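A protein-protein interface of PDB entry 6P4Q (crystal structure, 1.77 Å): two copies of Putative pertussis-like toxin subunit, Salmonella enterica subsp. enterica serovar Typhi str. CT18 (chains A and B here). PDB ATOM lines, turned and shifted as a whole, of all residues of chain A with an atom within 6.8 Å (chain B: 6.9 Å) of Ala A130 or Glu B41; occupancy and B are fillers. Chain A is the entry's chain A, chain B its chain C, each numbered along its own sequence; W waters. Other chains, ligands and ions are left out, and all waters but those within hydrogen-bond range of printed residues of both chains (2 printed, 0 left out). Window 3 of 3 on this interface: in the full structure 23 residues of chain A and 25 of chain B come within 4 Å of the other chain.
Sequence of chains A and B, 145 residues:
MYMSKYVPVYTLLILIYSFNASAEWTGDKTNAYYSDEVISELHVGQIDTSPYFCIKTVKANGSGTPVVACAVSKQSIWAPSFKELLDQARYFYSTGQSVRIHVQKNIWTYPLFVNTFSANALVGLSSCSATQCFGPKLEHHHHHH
O of Leu B42 touches C of Ser A126 (3.9 Å). Ser A127 touches Tyr B93. N of Cys A128 touches OE1 of Glu B41, 3.8 Å away. Ala A130 touches Glu B41. CB of Glu B41 touches CG of Phe A134 (3.4 Å). CD2 of Phe A134 touches N of Leu B42, at 3.8 Å. O of Phe A134 touches CB of His B43 (3.3 Å). Cys B54 touches Phe A134. Ile B55 touches Phe A134. Phe A134 touches Lys B56.
Ala A130 touches just one residue of chain B: Glu B41 (3.5 Å). Of the printed residues of chain A, His B43 touches Ser A126 and Phe A134. Printed residues of chain B within 4 Å of Ser A129: Ser B40 and Glu B41. Of the printed residues of chain B, Gln A97 touches Tyr B93. Of the printed residues of chain B, Ser A127 touches Glu B41 (2.7 Å), Leu B42 (2.9 Å) and Tyr B93 (3.6 Å). Thr A131 touches none of the printed residues of chain B.
Water W1 lies within hydrogen-bond range of the side-chain hydroxyl (OH) of Tyr B93, the backbone carbonyl oxygen (O) of Ser B40, the side-chain hydroxyl (OG) of Ser A129 and the side-chain carboxylate (OE1) of Glu B41. Water W2 lies within hydrogen-bond range of O of Gln A132 (2.5 Å), N of Ala A130 (2.9 Å), OE2 of Glu B41 (3.1 Å) and N of Ser A129 (3.1 Å).
No position is printed for both chains. Of the 16 pairs that touch across the chains among the printed residues, none has its exchanged pair printed and touching as well.
O of Ser B40 is in hydrogen-bond range of OG of Ser A129, 3.2 Å away. The side-chain carboxylate of Glu B41 sits at hydrogen-bond distance from the side-chain hydroxyl of Ser A129 (2.7 Å). OG of Ser A127 lies within hydrogen-bond range of N of Leu B42 (2.9 Å). The side-chain hydroxyl of Ser A126 lies within hydrogen-bond range of a ring nitrogen (ND1) of His B43 (2.8 Å). The side-chain hydroxyl (OG) of Ser A127 lies within hydrogen-bond range of the side-chain carboxylate (OE1) of Glu B41 (2.7 Å). The side-chain amide nitrogen (NE2) of Gln A97 lies within hydrogen-bond range of the side-chain hydroxyl (OH) of Tyr B93, at 2.8 Å.
The backbone carbonyl oxygen of Phe A134 lies close to the side-chain hydroxyl of Ser A126, at 3.3 Å. The side-chain sulfur (SG) of Cys A128 is disulfide-bonded to the side-chain sulfur (SG) of Cys A133 (2.0 Å). The backbone carbonyl oxygen (O) of Ser A98 lies within hydrogen-bond range of the backbone NH (N) of Cys A128 (3.2 Å). O of Cys B54 is in hydrogen-bond range of N of His B43. N of Ser B40 sits at hydrogen-bond distance from O of Lys B56, 2.8 Å away. The backbone carbonyl oxygen of Ser A127 lies within hydrogen-bond range of the backbone NH of Phe A134 (2.8 Å).
Printed residues of chain B that touch a printed residue of chain A: Ser B40, Glu B41, Leu B42, His B43, Cys B54, Ile B55, Lys B56 and Tyr B93. Hydrophobic or aromatic side chains of chain B that line the printed part of chain A: His B43 and Tyr B93. Of the 12 printed residues of chain A, 7 touch a printed residue of chain B. Printed residues of chain A that touch a printed residue of chain B: Gln A97, Ser A126, Ser A127, Cys A128, Ser A129, Ala A130 and Phe A134. Hydrophobic or aromatic side chains of chain A within 4 Å of the printed part of chain B: Ala A130 and Phe A134. Among the printed residues, 16 pairs touch across the chains. Among the printed residues, no Asp or Glu carboxylate lies within 4 Å of a Lys or Arg side-chain nitrogen of the other chain.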
ATOM      1  N   ASP A  36       9.742   9.523   2.078  1.00  0.00           N
ATOM      2  CA  ASP A  36      10.149  10.710   1.313  1.00  0.00           C
ATOM      3  C   ASP A  36       9.445  11.961   1.827  1.00  0.00           C
ATOM      4  O   ASP A  36       9.056  12.839   1.052  1.00  0.00           O
ATOM      5  CB  ASP A  36       9.886  10.525  -0.184  1.00  0.00           C
ATOM      6  CG  ASP A  36      10.329   9.164  -0.689  1.00  0.00           C
ATOM      7  OD1 ASP A  36      11.467   8.768  -0.379  1.00  0.00           O
ATOM      8  OD2 ASP A  36       9.532   8.506  -1.390  1.00  0.00           O
ATOM      9  N   GLN A  97      15.737  17.026   6.739  1.00  0.00           N
ATOM     10  CA  GLN A  97      16.117  15.921   5.875  1.00  0.00           C
ATOM     11  C   GLN A  97      14.923  15.006   5.596  1.00  0.00           C
ATOM     12  O   GLN A  97      13.929  14.971   6.337  1.00  0.00           O
ATOM     13  CB  GLN A  97      17.254  15.110   6.499  1.00  0.00           C
ATOM     14  CG  GLN A  97      16.782  14.275   7.676  1.00  0.00           C
ATOM     15  CD  GLN A  97      17.934  13.811   8.530  1.00  0.00           C
ATOM     16  OE1 GLN A  97      18.400  14.538   9.409  1.00  0.00           O
ATOM     17  NE2 GLN A  97      18.418  12.601   8.265  1.00  0.00           N
ATOM     18  N   SER A  98      15.029  14.262   4.498  1.00  0.00           N
ATOM     19  CA  SER A  98      13.973  13.331   4.120  1.00  0.00           C
ATOM     20  C   SER A  98      13.877  12.190   5.122  1.00  0.00           C
ATOM     21  O   SER A  98      14.893  11.671   5.593  1.00  0.00           O
ATOM     22  CB  SER A  98      14.247  12.767   2.727  1.00  0.00           C
ATOM     23  OG  SER A  98      14.125  13.771   1.738  1.00  0.00           O
ATOM     24  N   SER A 126      12.308   7.128  10.381  1.00  0.00           N
ATOM     25  CA  SER A 126      13.427   6.534   9.658  1.00  0.00           C
ATOM     26  C   SER A 126      14.082   7.597   8.784  1.00  0.00           C
ATOM     27  O   SER A 126      13.388   8.319   8.066  1.00  0.00           O
ATOM     28  CB  SER A 126      12.966   5.375   8.770  1.00  0.00           C
ATOM     29  OG  SER A 126      12.212   4.410   9.485  1.00  0.00           O
ATOM     30  N   SER A 127      15.406   7.668   8.820  1.00  0.00           N
ATOM     31  CA  SER A 127      16.080   8.497   7.828  1.00  0.00           C
ATOM     32  C   SER A 127      15.910   7.880   6.439  1.00  0.00           C
ATOM     33  O   SER A 127      15.643   6.681   6.282  1.00  0.00           O
ATOM     34  CB  SER A 127      17.562   8.671   8.181  1.00  0.00           C
ATOM     35  OG  SER A 127      18.239   7.429   8.139  1.00  0.00           O
ATOM     36  N   CYS A 128      16.016   8.732   5.417  1.00  0.00           N
ATOM     37  CA  CYS A 128      15.816   8.334   4.018  1.00  0.00           C
ATOM     38  C   CYS A 128      16.853   9.009   3.132  1.00  0.00           C
ATOM     39  O   CYS A 128      16.513   9.693   2.174  1.00  0.00           O
ATOM     40  CB  CYS A 128      14.471   8.746   3.432  1.00  0.00           C
ATOM     41  SG  CYS A 128      13.033   8.213   4.184  1.00  0.00           S
ATOM     42  N   SER A 129      18.124   8.840   3.446  1.00  0.00           N
ATOM     43  CA  SER A 129      19.138   9.582   2.710  1.00  0.00           C
ATOM     44  C   SER A 129      19.623   8.862   1.459  1.00  0.00           C
ATOM     45  O   SER A 129      20.467   9.408   0.737  1.00  0.00           O
ATOM     46  CB  SER A 129      20.320   9.892   3.622  1.00  0.00           C
ATOM     47  OG  SER A 129      21.136   8.742   3.778  1.00  0.00           O
ATOM     48  N   ALA A 130      19.108   7.667   1.177  1.00  0.00           N
ATOM     49  CA  ALA A 130      19.516   6.913  -0.004  1.00  0.00           C
ATOM     50  C   ALA A 130      18.297   6.497  -0.821  1.00  0.00           C
ATOM     51  O   ALA A 130      17.278   7.196  -0.821  1.00  0.00           O
ATOM     52  CB  ALA A 130      20.346   5.693   0.397  1.00  0.00           C
ATOM     53  N   THR A 131      18.373   5.361  -1.518  1.00  0.00           N
ATOM     54  CA  THR A 131      17.307   5.036  -2.462  1.00  0.00           C
ATOM     55  C   THR A 131      16.029   4.617  -1.746  1.00  0.00           C
ATOM     56  O   THR A 131      14.932   5.030  -2.132  1.00  0.00           O
ATOM     57  CB  THR A 131      17.765   3.943  -3.426  1.00  0.00           C
ATOM     58  OG1 THR A 131      18.880   4.431  -4.185  1.00  0.00           O
ATOM     59  CG2 THR A 131      16.645   3.575  -4.375  1.00  0.00           C
ATOM     60  N   GLN A 132      16.153   3.802  -0.708  1.00  0.00           N
ATOM     61  CA  GLN A 132      15.029   3.369   0.110  1.00  0.00           C
ATOM     62  C   GLN A 132      15.250   3.869   1.527  1.00  0.00           C
ATOM     63  O   GLN A 132      16.389   3.908   2.003  1.00  0.00           O
ATOM     64  CB  GLN A 132      14.896   1.839   0.118  1.00  0.00           C
ATOM     65  CG  GLN A 132      14.630   1.210  -1.257  1.00  0.00           C
ATOM     66  CD  GLN A 132      13.211   1.435  -1.750  1.00  0.00           C
ATOM     67  OE1 GLN A 132      12.334   1.881  -1.001  1.00  0.00           O
ATOM     68  NE2 GLN A 132      12.976   1.130  -3.022  1.00  0.00           N
ATOM     69  N   CYS A 133      14.172   4.256   2.202  1.00  0.00           N
ATOM     70  CA  CYS A 133      14.306   4.725   3.577  1.00  0.00           C
ATOM     71  C   CYS A 133      14.791   3.603   4.481  1.00  0.00           C
ATOM     72  O   CYS A 133      14.498   2.429   4.263  1.00  0.00           O
ATOM     73  CB  CYS A 133      12.978   5.262   4.089  1.00  0.00           C
ATOM     74  SG  CYS A 133      12.370   6.625   3.104  1.00  0.00           S
ATOM     75  N   PHE A 134      15.546   3.979   5.514  1.00  0.00           N
ATOM     76  CA  PHE A 134      16.157   3.013   6.420  1.00  0.00           C
ATOM     77  C   PHE A 134      15.137   2.674   7.495  1.00  0.00           C
ATOM     78  O   PHE A 134      15.194   3.155   8.626  1.00  0.00           O
ATOM     79  CB  PHE A 134      17.432   3.587   7.028  1.00  0.00           C
ATOM     80  CG  PHE A 134      18.109   2.672   8.002  1.00  0.00           C
ATOM     81  CD1 PHE A 134      18.585   1.439   7.589  1.00  0.00           C
ATOM     82  CD2 PHE A 134      18.276   3.043   9.338  1.00  0.00           C
ATOM     83  CE1 PHE A 134      19.227   0.584   8.487  1.00  0.00           C
ATOM     84  CE2 PHE A 134      18.917   2.197  10.233  1.00  0.00           C
ATOM     85  CZ  PHE A 134      19.396   0.971   9.801  1.00  0.00           C
ATOM     86  N   VAL B  38      31.188   5.103   8.496  1.00  0.00           N
ATOM     87  CA  VAL B  38      30.459   6.336   8.784  1.00  0.00           C
ATOM     88  C   VAL B  38      28.987   5.987   8.938  1.00  0.00           C
ATOM     89  O   VAL B  38      28.433   5.253   8.109  1.00  0.00           O
ATOM     90  CB  VAL B  38      30.634   7.392   7.677  1.00  0.00           C
ATOM     91  CG1 VAL B  38      29.767   8.617   7.982  1.00  0.00           C
ATOM     92  CG2 VAL B  38      32.094   7.792   7.540  1.00  0.00           C
ATOM     93  N   ILE B  39      28.355   6.500   9.998  1.00  0.00           N
ATOM     94  CA  ILE B  39      26.925   6.270  10.195  1.00  0.00           C
ATOM     95  C   ILE B  39      26.154   7.096   9.175  1.00  0.00           C
ATOM     96  O   ILE B  39      26.218   8.329   9.185  1.00  0.00           O
ATOM     97  CB  ILE B  39      26.490   6.627  11.624  1.00  0.00           C
ATOM     98  CG1 ILE B  39      27.282   5.823  12.663  1.00  0.00           C
ATOM     99  CG2 ILE B  39      24.992   6.383  11.807  1.00  0.00           C
ATOM    100  CD1 ILE B  39      27.019   6.282  14.113  1.00  0.00           C
ATOM    101  N   SER B  40      25.406   6.414   8.301  1.00  0.00           N
ATOM    102  CA  SER B  40      24.735   7.061   7.188  1.00  0.00           C
ATOM    103  C   SER B  40      23.221   7.033   7.283  1.00  0.00           C
ATOM    104  O   SER B  40      22.561   7.735   6.510  1.00  0.00           O
ATOM    105  CB  SER B  40      25.170   6.411   5.864  1.00  0.00           C
ATOM    106  OG  SER B  40      24.762   5.062   5.808  1.00  0.00           O
ATOM    107  N   GLU B  41      22.653   6.237   8.191  1.00  0.00           N
ATOM    108  CA  GLU B  41      21.210   6.209   8.405  1.00  0.00           C
ATOM    109  C   GLU B  41      20.950   5.947   9.880  1.00  0.00           C
ATOM    110  O   GLU B  41      21.758   5.304  10.560  1.00  0.00           O
ATOM    111  CB  GLU B  41      20.499   5.116   7.590  1.00  0.00           C
ATOM    112  CG  GLU B  41      20.868   5.025   6.116  1.00  0.00           C
ATOM    113  CD  GLU B  41      20.190   6.079   5.255  1.00  0.00           C
ATOM    114  OE1 GLU B  41      19.326   6.827   5.759  1.00  0.00           O
ATOM    115  OE2 GLU B  41      20.524   6.148   4.055  1.00  0.00           O
ATOM    116  N   LEU B  42      19.787   6.402  10.348  1.00  0.00           N
ATOM    117  CA  LEU B  42      19.368   6.236  11.733  1.00  0.00           C
ATOM    118  C   LEU B  42      17.856   6.040  11.757  1.00  0.00           C
ATOM    119  O   LEU B  42      17.125   6.732  11.046  1.00  0.00           O
ATOM    120  CB  LEU B  42      19.778   7.465  12.558  1.00  0.00           C
ATOM    121  CG  LEU B  42      19.298   7.610  13.997  1.00  0.00           C
ATOM    122  CD1 LEU B  42      19.886   6.518  14.842  1.00  0.00           C
ATOM    123  CD2 LEU B  42      19.719   8.988  14.520  1.00  0.00           C
ATOM    124  N   HIS B  43      17.386   5.099  12.572  1.00  0.00           N
ATOM    125  CA  HIS B  43      15.964   4.799  12.687  1.00  0.00           C
ATOM    126  C   HIS B  43      15.619   4.642  14.158  1.00  0.00           C
ATOM    127  O   HIS B  43      16.398   4.049  14.905  1.00  0.00           O
ATOM    128  CB  HIS B  43      15.605   3.504  11.921  1.00  0.00           C
ATOM    129  CG  HIS B  43      14.327   2.859  12.372  1.00  0.00           C
ATOM    130  ND1 HIS B  43      13.125   3.040  11.719  1.00  0.00           N
ATOM    131  CD2 HIS B  43      14.070   2.005  13.395  1.00  0.00           C
ATOM    132  CE1 HIS B  43      12.181   2.348  12.334  1.00  0.00           C
ATOM    133  NE2 HIS B  43      12.732   1.700  13.345  1.00  0.00           N
ATOM    134  N   CYS B  54      18.262   1.741  15.376  1.00  0.00           N
ATOM    135  CA  CYS B  54      19.169   1.042  14.482  1.00  0.00           C
ATOM    136  C   CYS B  54      19.970   2.066  13.699  1.00  0.00           C
ATOM    137  O   CYS B  54      19.499   3.175  13.433  1.00  0.00           O
ATOM    138  CB  CYS B  54      18.431   0.145  13.478  1.00  0.00           C
ATOM    139  SG  CYS B  54      17.352  -1.081  14.219  1.00  0.00           S
ATOM    140  N   ILE B  55      21.195   1.690  13.349  1.00  0.00           N
ATOM    141  CA  ILE B  55      22.017   2.518  12.479  1.00  0.00           C
ATOM    142  C   ILE B  55      22.538   1.660  11.342  1.00  0.00           C
ATOM    143  O   ILE B  55      22.681   0.435  11.462  1.00  0.00           O
ATOM    144  CB  ILE B  55      23.198   3.178  13.230  1.00  0.00           C
ATOM    145  CG1 ILE B  55      24.017   2.132  13.986  1.00  0.00           C
ATOM    146  CG2 ILE B  55      22.689   4.248  14.188  1.00  0.00           C
ATOM    147  CD1 ILE B  55      25.219   2.773  14.661  1.00  0.00           C
ATOM    148  N   LYS B  56      22.834   2.328  10.234  1.00  0.00           N
ATOM    149  CA  LYS B  56      23.548   1.762   9.106  1.00  0.00           C
ATOM    150  C   LYS B  56      24.852   2.527   8.986  1.00  0.00           C
ATOM    151  O   LYS B  56      24.859   3.759   9.097  1.00  0.00           O
ATOM    152  CB  LYS B  56      22.734   1.889   7.811  1.00  0.00           C
ATOM    153  CG  LYS B  56      23.468   1.415   6.580  1.00  0.00           C
ATOM    154  CD  LYS B  56      22.475   1.266   5.430  1.00  0.00           C
ATOM    155  CE  LYS B  56      23.167   1.257   4.077  1.00  0.00           C
ATOM    156  NZ  LYS B  56      22.172   1.207   2.957  1.00  0.00           N
ATOM    157  N   THR B  57      25.955   1.801   8.813  1.00  0.00           N
ATOM    158  CA  THR B  57      27.238   2.425   8.536  1.00  0.00           C
ATOM    159  C   THR B  57      27.762   1.936   7.193  1.00  0.00           C
ATOM    160  O   THR B  57      27.506   0.803   6.781  1.00  0.00           O
ATOM    161  CB  THR B  57      28.279   2.144   9.647  1.00  0.00           C
ATOM    162  OG1 THR B  57      28.751   0.794   9.560  1.00  0.00           O
ATOM    163  CG2 THR B  57      27.669   2.367  11.030  1.00  0.00           C
ATOM    164  N   TYR B  93      26.673  10.320  13.791  1.00  0.00           N
ATOM    165  CA  TYR B  93      25.863  10.523  12.596  1.00  0.00           C
ATOM    166  C   TYR B  93      25.883  11.987  12.168  1.00  0.00           C
ATOM    167  O   TYR B  93      26.029  12.299  10.978  1.00  0.00           O
ATOM    168  CB  TYR B  93      24.439  10.040  12.893  1.00  0.00           C
ATOM    169  CG  TYR B  93      23.375  10.252  11.842  1.00  0.00           C
ATOM    170  CD1 TYR B  93      23.549   9.819  10.526  1.00  0.00           C
ATOM    171  CD2 TYR B  93      22.159  10.834  12.189  1.00  0.00           C
ATOM    172  CE1 TYR B  93      22.540   9.990   9.578  1.00  0.00           C
ATOM    173  CE2 TYR B  93      21.153  11.000  11.258  1.00  0.00           C
ATOM    174  CZ  TYR B  93      21.346  10.579   9.961  1.00  0.00           C
ATOM    175  OH  TYR B  93      20.346  10.754   9.047  1.00  0.00           O
HETATM  176  O   HOH W   1      20.654   9.746   6.854  1.00  0.00           O
HETATM  177  O   HOH W   2      17.694   5.786   2.918  1.00  0.00           O
